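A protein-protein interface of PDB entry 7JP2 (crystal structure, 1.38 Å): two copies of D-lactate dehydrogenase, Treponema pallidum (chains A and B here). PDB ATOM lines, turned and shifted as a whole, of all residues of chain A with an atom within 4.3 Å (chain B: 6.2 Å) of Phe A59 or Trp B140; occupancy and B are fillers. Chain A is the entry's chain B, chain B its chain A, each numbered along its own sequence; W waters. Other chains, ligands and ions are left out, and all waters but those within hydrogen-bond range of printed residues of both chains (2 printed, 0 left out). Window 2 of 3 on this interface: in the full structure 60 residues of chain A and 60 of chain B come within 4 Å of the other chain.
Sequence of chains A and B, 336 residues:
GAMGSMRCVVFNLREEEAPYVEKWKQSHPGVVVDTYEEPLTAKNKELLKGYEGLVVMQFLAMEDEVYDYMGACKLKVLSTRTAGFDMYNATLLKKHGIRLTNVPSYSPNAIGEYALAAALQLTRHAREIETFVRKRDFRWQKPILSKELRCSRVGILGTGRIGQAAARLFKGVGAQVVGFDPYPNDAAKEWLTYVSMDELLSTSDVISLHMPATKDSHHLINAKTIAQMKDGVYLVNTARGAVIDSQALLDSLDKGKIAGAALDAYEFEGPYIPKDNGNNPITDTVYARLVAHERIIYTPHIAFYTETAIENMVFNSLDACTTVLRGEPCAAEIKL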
ATOM      1  N   ARG A  14      29.376  19.457 -22.984  1.00  0.00           N
ATOM      2  CA  ARG A  14      29.259  18.669 -24.200  1.00  0.00           C
ATOM      3  C   ARG A  14      29.302  19.569 -25.429  1.00  0.00           C
ATOM      4  O   ARG A  14      29.041  20.771 -25.357  1.00  0.00           O
ATOM      5  CB  ARG A  14      27.963  17.857 -24.175  1.00  0.00           C
ATOM      6  CG  ARG A  14      27.840  16.955 -22.943  1.00  0.00           C
ATOM      7  CD  ARG A  14      26.691  15.921 -23.057  1.00  0.00           C
ATOM      8  NE  ARG A  14      25.483  16.577 -23.543  1.00  0.00           N
ATOM      9  CZ  ARG A  14      24.696  17.351 -22.802  1.00  0.00           C
ATOM     10  NH1 ARG A  14      24.942  17.528 -21.505  1.00  0.00           N
ATOM     11  NH2 ARG A  14      23.657  17.948 -23.366  1.00  0.00           N
ATOM     12  N   GLU A  16      27.414  20.117 -27.924  1.00  0.00           N
ATOM     13  CA  GLU A  16      26.244  20.911 -28.286  1.00  0.00           C
ATOM     14  C   GLU A  16      25.961  22.027 -27.289  1.00  0.00           C
ATOM     15  O   GLU A  16      25.253  22.982 -27.632  1.00  0.00           O
ATOM     16  CB  GLU A  16      25.026  20.003 -28.463  1.00  0.00           C
ATOM     17  CG  GLU A  16      24.494  19.340 -27.184  1.00  0.00           C
ATOM     18  CD  GLU A  16      25.120  17.999 -26.851  1.00  0.00           C
ATOM     19  OE1 GLU A  16      26.231  17.706 -27.341  1.00  0.00           O
ATOM     20  OE2 GLU A  16      24.481  17.239 -26.083  1.00  0.00           O
ATOM     21  N   MET A  57      26.489  18.987 -14.980  1.00  0.00           N
ATOM     22  CA  MET A  57      25.509  18.060 -15.529  1.00  0.00           C
ATOM     23  C   MET A  57      26.233  16.716 -15.562  1.00  0.00           C
ATOM     24  O   MET A  57      26.711  16.229 -16.585  1.00  0.00           O
ATOM     25  CB  MET A  57      25.023  18.467 -16.918  1.00  0.00           C
ATOM     26  CG  MET A  57      23.971  17.530 -17.471  1.00  0.00           C
ATOM     27  SD  MET A  57      23.088  18.331 -18.819  1.00  0.00           S
ATOM     28  CE  MET A  57      22.169  16.925 -19.454  1.00  0.00           C
ATOM     29  N   GLN A  58      26.386  16.119 -14.391  1.00  0.00           N
ATOM     30  CA  GLN A  58      27.316  15.023 -14.213  1.00  0.00           C
ATOM     31  C   GLN A  58      26.574  13.737 -13.896  1.00  0.00           C
ATOM     32  O   GLN A  58      25.686  13.719 -13.042  1.00  0.00           O
ATOM     33  CB  GLN A  58      28.325  15.361 -13.120  1.00  0.00           C
ATOM     34  CG  GLN A  58      29.365  14.279 -12.960  1.00  0.00           C
ATOM     35  CD  GLN A  58      30.666  14.794 -12.408  1.00  0.00           C
ATOM     36  OE1 GLN A  58      31.171  15.836 -12.827  1.00  0.00           O
ATOM     37  NE2 GLN A  58      31.234  14.054 -11.468  1.00  0.00           N
ATOM     38  N   PHE A  59      26.979  12.663 -14.577  1.00  0.00           N
ATOM     39  CA  PHE A  59      26.360  11.348 -14.513  1.00  0.00           C
ATOM     40  C   PHE A  59      27.113  10.395 -13.610  1.00  0.00           C
ATOM     41  O   PHE A  59      26.732   9.229 -13.495  1.00  0.00           O
ATOM     42  CB  PHE A  59      26.287  10.793 -15.934  1.00  0.00           C
ATOM     43  CG  PHE A  59      25.571  11.707 -16.864  1.00  0.00           C
ATOM     44  CD1 PHE A  59      24.223  11.947 -16.673  1.00  0.00           C
ATOM     45  CD2 PHE A  59      26.233  12.374 -17.884  1.00  0.00           C
ATOM     46  CE1 PHE A  59      23.532  12.802 -17.495  1.00  0.00           C
ATOM     47  CE2 PHE A  59      25.546  13.242 -18.716  1.00  0.00           C
ATOM     48  CZ  PHE A  59      24.195  13.454 -18.520  1.00  0.00           C
ATOM     49  N   LEU A  60      28.151  10.883 -12.950  1.00  0.00           N
ATOM     50  CA  LEU A  60      29.070  10.094 -12.150  1.00  0.00           C
ATOM     51  C   LEU A  60      29.133  10.736 -10.778  1.00  0.00           C
ATOM     52  O   LEU A  60      29.300  11.953 -10.677  1.00  0.00           O
ATOM     53  CB  LEU A  60      30.434  10.154 -12.834  1.00  0.00           C
ATOM     54  CG  LEU A  60      31.708   9.800 -12.080  1.00  0.00           C
ATOM     55  CD1 LEU A  60      31.746   8.311 -11.844  1.00  0.00           C
ATOM     56  CD2 LEU A  60      32.923  10.278 -12.869  1.00  0.00           C
ATOM     57  N   ILE A 273      21.412   4.831 -18.306  1.00  0.00           N
ATOM     58  CA  ILE A 273      21.031   6.045 -19.019  1.00  0.00           C
ATOM     59  C   ILE A 273      21.840   7.198 -18.446  1.00  0.00           C
ATOM     60  O   ILE A 273      21.878   7.363 -17.226  1.00  0.00           O
ATOM     61  CB  ILE A 273      19.527   6.347 -18.875  1.00  0.00           C
ATOM     62  CG1 ILE A 273      18.688   5.326 -19.643  1.00  0.00           C
ATOM     63  CG2 ILE A 273      19.201   7.776 -19.300  1.00  0.00           C
ATOM     64  CD1 ILE A 273      18.789   5.441 -21.145  1.00  0.00           C
ATOM     65  N   PRO A 274      22.476   8.048 -19.282  1.00  0.00           N
ATOM     66  CA  PRO A 274      22.627   7.983 -20.742  1.00  0.00           C
ATOM     67  C   PRO A 274      24.039   7.509 -21.107  1.00  0.00           C
ATOM     68  O   PRO A 274      24.934   8.312 -21.349  1.00  0.00           O
ATOM     69  CB  PRO A 274      22.414   9.436 -21.166  1.00  0.00           C
ATOM     70  CG  PRO A 274      22.911  10.253 -19.999  1.00  0.00           C
ATOM     71  CD  PRO A 274      22.975   9.338 -18.773  1.00  0.00           C
ATOM     72  N   PRO A 300      16.200   6.309 -25.596  1.00  0.00           N
ATOM     73  CA  PRO A 300      16.974   6.458 -24.350  1.00  0.00           C
ATOM     74  C   PRO A 300      16.803   7.825 -23.690  1.00  0.00           C
ATOM     75  O   PRO A 300      17.774   8.556 -23.450  1.00  0.00           O
ATOM     76  CB  PRO A 300      18.412   6.234 -24.833  1.00  0.00           C
ATOM     77  CG  PRO A 300      18.407   6.796 -26.231  1.00  0.00           C
ATOM     78  CD  PRO A 300      17.062   6.390 -26.793  1.00  0.00           C
ATOM     79  N   HIS A 301      15.556   8.177 -23.388  1.00  0.00           N
ATOM     80  CA  HIS A 301      15.262   9.366 -22.593  1.00  0.00           C
ATOM     81  C   HIS A 301      15.689  10.628 -23.339  1.00  0.00           C
ATOM     82  O   HIS A 301      16.368  11.504 -22.799  1.00  0.00           O
ATOM     83  CB  HIS A 301      15.931   9.236 -21.230  1.00  0.00           C
ATOM     84  CG  HIS A 301      15.331  10.084 -20.163  1.00  0.00           C
ATOM     85  ND1 HIS A 301      14.986   9.582 -18.927  1.00  0.00           N
ATOM     86  CD2 HIS A 301      15.065  11.409 -20.124  1.00  0.00           C
ATOM     87  CE1 HIS A 301      14.525  10.566 -18.175  1.00  0.00           C
ATOM     88  NE2 HIS A 301      14.558  11.684 -18.878  1.00  0.00           N
ATOM     89  N   ILE A 302      15.266  10.709 -24.606  1.00  0.00           N
ATOM     90  CA  ILE A 302      15.656  11.779 -25.511  1.00  0.00           C
ATOM     91  C   ILE A 302      14.481  12.653 -25.949  1.00  0.00           C
ATOM     92  O   ILE A 302      14.639  13.487 -26.837  1.00  0.00           O
ATOM     93  CB  ILE A 302      16.447  11.264 -26.732  1.00  0.00           C
ATOM     94  CG1 ILE A 302      15.766  10.066 -27.415  1.00  0.00           C
ATOM     95  CG2 ILE A 302      17.869  10.899 -26.322  1.00  0.00           C
ATOM     96  CD1 ILE A 302      14.408  10.354 -28.053  1.00  0.00           C
ATOM     97  N   PHE A 304      13.392  15.203 -24.565  1.00  0.00           N
ATOM     98  CA  PHE A 304      13.829  16.571 -24.334  1.00  0.00           C
ATOM     99  C   PHE A 304      14.916  17.036 -25.294  1.00  0.00           C
ATOM    100  O   PHE A 304      15.232  18.232 -25.299  1.00  0.00           O
ATOM    101  CB  PHE A 304      14.407  16.701 -22.914  1.00  0.00           C
ATOM    102  CG  PHE A 304      15.864  16.272 -22.795  1.00  0.00           C
ATOM    103  CD1 PHE A 304      16.209  14.934 -22.771  1.00  0.00           C
ATOM    104  CD2 PHE A 304      16.879  17.215 -22.725  1.00  0.00           C
ATOM    105  CE1 PHE A 304      17.527  14.535 -22.690  1.00  0.00           C
ATOM    106  CE2 PHE A 304      18.201  16.827 -22.638  1.00  0.00           C
ATOM    107  CZ  PHE A 304      18.523  15.481 -22.623  1.00  0.00           C
ATOM    108  N   TYR A 305      15.533  16.136 -26.060  1.00  0.00           N
ATOM    109  CA  TYR A 305      16.885  16.372 -26.582  1.00  0.00           C
ATOM    110  C   TYR A 305      16.836  17.144 -27.901  1.00  0.00           C
ATOM    111  O   TYR A 305      17.018  16.605 -28.992  1.00  0.00           O
ATOM    112  CB  TYR A 305      17.622  15.037 -26.680  1.00  0.00           C
ATOM    113  CG  TYR A 305      19.110  15.135 -26.926  1.00  0.00           C
ATOM    114  CD1 TYR A 305      19.929  15.878 -26.085  1.00  0.00           C
ATOM    115  CD2 TYR A 305      19.700  14.478 -27.991  1.00  0.00           C
ATOM    116  CE1 TYR A 305      21.296  15.966 -26.312  1.00  0.00           C
ATOM    117  CE2 TYR A 305      21.057  14.556 -28.221  1.00  0.00           C
ATOM    118  CZ  TYR A 305      21.855  15.300 -27.388  1.00  0.00           C
ATOM    119  OH  TYR A 305      23.208  15.363 -27.660  1.00  0.00           O
ATOM    120  N   PHE B 138      23.101   4.273 -25.419  1.00  0.00           N
ATOM    121  CA  PHE B 138      22.030   5.112 -24.902  1.00  0.00           C
ATOM    122  C   PHE B 138      22.514   6.526 -24.583  1.00  0.00           C
ATOM    123  O   PHE B 138      21.945   7.200 -23.720  1.00  0.00           O
ATOM    124  CB  PHE B 138      21.392   4.482 -23.661  1.00  0.00           C
ATOM    125  CG  PHE B 138      20.701   3.146 -23.884  1.00  0.00           C
ATOM    126  CD1 PHE B 138      20.397   2.652 -25.147  1.00  0.00           C
ATOM    127  CD2 PHE B 138      20.316   2.400 -22.775  1.00  0.00           C
ATOM    128  CE1 PHE B 138      19.739   1.425 -25.289  1.00  0.00           C
ATOM    129  CE2 PHE B 138      19.659   1.196 -22.911  1.00  0.00           C
ATOM    130  CZ  PHE B 138      19.378   0.699 -24.173  1.00  0.00           C
ATOM    131  N   ARG B 139      23.547   6.995 -25.265  1.00  0.00           N
ATOM    132  CA  ARG B 139      24.086   8.313 -24.985  1.00  0.00           C
ATOM    133  C   ARG B 139      23.209   9.426 -25.545  1.00  0.00           C
ATOM    134  O   ARG B 139      22.516   9.272 -26.556  1.00  0.00           O
ATOM    135  CB  ARG B 139      25.486   8.446 -25.579  1.00  0.00           C
ATOM    136  CG  ARG B 139      26.536   7.654 -24.835  1.00  0.00           C
ATOM    137  CD  ARG B 139      27.904   7.768 -25.492  1.00  0.00           C
ATOM    138  NE  ARG B 139      27.917   7.120 -26.800  1.00  0.00           N
ATOM    139  CZ  ARG B 139      28.946   7.131 -27.639  1.00  0.00           C
ATOM    140  NH1 ARG B 139      30.063   7.766 -27.313  1.00  0.00           N
ATOM    141  NH2 ARG B 139      28.854   6.505 -28.803  1.00  0.00           N
ATOM    142  N   TRP B 140      23.259  10.569 -24.869  1.00  0.00           N
ATOM    143  CA  TRP B 140      22.720  11.826 -25.387  1.00  0.00           C
ATOM    144  C   TRP B 140      23.850  12.446 -26.192  1.00  0.00           C
ATOM    145  O   TRP B 140      24.745  13.098 -25.659  1.00  0.00           O
ATOM    146  CB  TRP B 140      22.277  12.713 -24.239  1.00  0.00           C
ATOM    147  CG  TRP B 140      21.188  12.098 -23.412  1.00  0.00           C
ATOM    148  CD1 TRP B 140      20.351  11.080 -23.776  1.00  0.00           C
ATOM    149  CD2 TRP B 140      20.815  12.467 -22.081  1.00  0.00           C
ATOM    150  NE1 TRP B 140      19.486  10.793 -22.749  1.00  0.00           N
ATOM    151  CE2 TRP B 140      19.743  11.636 -21.699  1.00  0.00           C
ATOM    152  CE3 TRP B 140      21.294  13.415 -21.169  1.00  0.00           C
ATOM    153  CZ2 TRP B 140      19.135  11.730 -20.441  1.00  0.00           C
ATOM    154  CZ3 TRP B 140      20.692  13.513 -19.933  1.00  0.00           C
ATOM    155  CH2 TRP B 140      19.623  12.675 -19.573  1.00  0.00           C
ATOM    156  N   GLN B 141      23.827  12.198 -27.502  1.00  0.00           N
ATOM    157  CA  GLN B 141      24.940  12.524 -28.381  1.00  0.00           C
ATOM    158  C   GLN B 141      24.456  13.300 -29.596  1.00  0.00           C
ATOM    159  O   GLN B 141      23.366  13.072 -30.112  1.00  0.00           O
ATOM    160  CB  GLN B 141      25.694  11.252 -28.792  1.00  0.00           C
ATOM    161  CG  GLN B 141      24.845  10.179 -29.455  1.00  0.00           C
ATOM    162  CD  GLN B 141      25.675   8.983 -29.879  1.00  0.00           C
ATOM    163  OE1 GLN B 141      26.757   9.134 -30.453  1.00  0.00           O
ATOM    164  NE2 GLN B 141      25.185   7.787 -29.580  1.00  0.00           N
ATOM    165  N   LYS B 142      25.311  14.209 -30.054  1.00  0.00           N
ATOM    166  CA  LYS B 142      24.964  15.151 -31.115  1.00  0.00           C
ATOM    167  C   LYS B 142      24.336  14.523 -32.348  1.00  0.00           C
ATOM    168  O   LYS B 142      23.423  15.145 -32.917  1.00  0.00           O
ATOM    169  CB  LYS B 142      26.237  15.946 -31.446  1.00  0.00           C
ATOM    170  CG  LYS B 142      26.185  16.774 -32.702  1.00  0.00           C
ATOM    171  CD  LYS B 142      25.270  17.963 -32.564  1.00  0.00           C
ATOM    172  CE  LYS B 142      25.437  18.869 -33.787  1.00  0.00           C
ATOM    173  NZ  LYS B 142      24.616  20.101 -33.717  1.00  0.00           N
ATOM    174  N   ILE B 144      22.057  12.522 -32.687  1.00  0.00           N
ATOM    175  CA  ILE B 144      20.622  12.350 -32.508  1.00  0.00           C
ATOM    176  C   ILE B 144      19.963  13.587 -31.909  1.00  0.00           C
ATOM    177  O   ILE B 144      18.786  13.537 -31.559  1.00  0.00           O
ATOM    178  CB  ILE B 144      20.248  11.073 -31.725  1.00  0.00           C
ATOM    179  CG1 ILE B 144      20.807  11.102 -30.294  1.00  0.00           C
ATOM    180  CG2 ILE B 144      20.685   9.835 -32.495  1.00  0.00           C
ATOM    181  CD1 ILE B 144      20.287   9.968 -29.390  1.00  0.00           C
HETATM  182  O   HOH W   1      25.222  10.671 -22.756  1.00  0.00           O
HETATM  183  O   HOH W   2      16.546  14.273 -30.324  1.00  0.00           O
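The backbone carbonyl oxygen (O) of Pro A300 lies within hydrogen-bond range of the indole nitrogen (NE1) of Trp B140 (2.9 Å). NE1 of Trp B140 is in hydrogen-bond range of O of His A301. The backbone carbonyl oxygen (O) of Trp B140 sits close to the side-chain hydroxyl (OH) of Tyr A305, at 3.4 Å. The backbone NH (N) of Gln B141 lies close to the side-chain hydroxyl (OH) of Tyr A305 (3.2 Å). OH of Tyr A305 lies within hydrogen-bond range of N of Lys B142, 3.4 Å away.
The side-chain hydroxyl (OH) of Tyr A305 is in hydrogen-bond range of the side-chain carboxylate (OE2) of Glu A16. The guanidinium group of Arg A14 is in hydrogen-bond range of the side-chain sulfur of Met A57 (3.4 Å).
Among the printed residues, pairs that only touch across the chains: Pro A274 with Phe B138 (3.2 Å), Pro A274 with Trp B140 (3.5 Å), Ile A302 with Trp B140 (3.6 Å), Pro A300 with Phe B138 (3.7 Å), Pro A274 with Arg B139 (3.7 Å), Ile A273 with Phe B138 (3.7 Å), Met A57 with Trp B140 (3.7 Å), Phe A304 with Trp B140 (3.7 Å), Phe A59 with Trp B140 (3.8 Å) and Tyr A305 with Ile B144 (3.8 Å).
Gln A58 touches none of the printed residues of chain B. Phe A59 touches just one residue of chain B: Trp B140. Printed residues of chain B within 4 Å of Pro A300: Phe B138 and Trp B140. Printed residues of chain B within 4 Å of Tyr A305: Trp B140 (3.3 Å), Gln B141 (3.1 Å), Lys B142 (3.4 Å) and Ile B144 (3.8 Å). Of chain A, only Met A57 (3.7 Å), Phe A59 (3.8 Å), Pro A274 (3.5 Å), Pro A300 (2.9 Å), His A301 (3.2 Å), Ile A302 (3.6 Å), Phe A304 (3.7 Å) and Tyr A305 (3.3 Å) come within 4 Å of Trp B140. The nearest printed residue of chain A that does not touch Trp B140 is Ile A273 (4.1 Å).
Among the printed residues, 15 pairs touch across the chains.
No position is printed for both chains. Of the 15 pairs that touch across the chains among the printed residues, none has its exchanged pair printed and touching as well.
Water W2 bridges the backbone carbonyl oxygen of Ile B144 and the backbone carbonyl oxygen of Tyr A305. Water W1 bridges O of Pro A274 and N of Trp B140.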
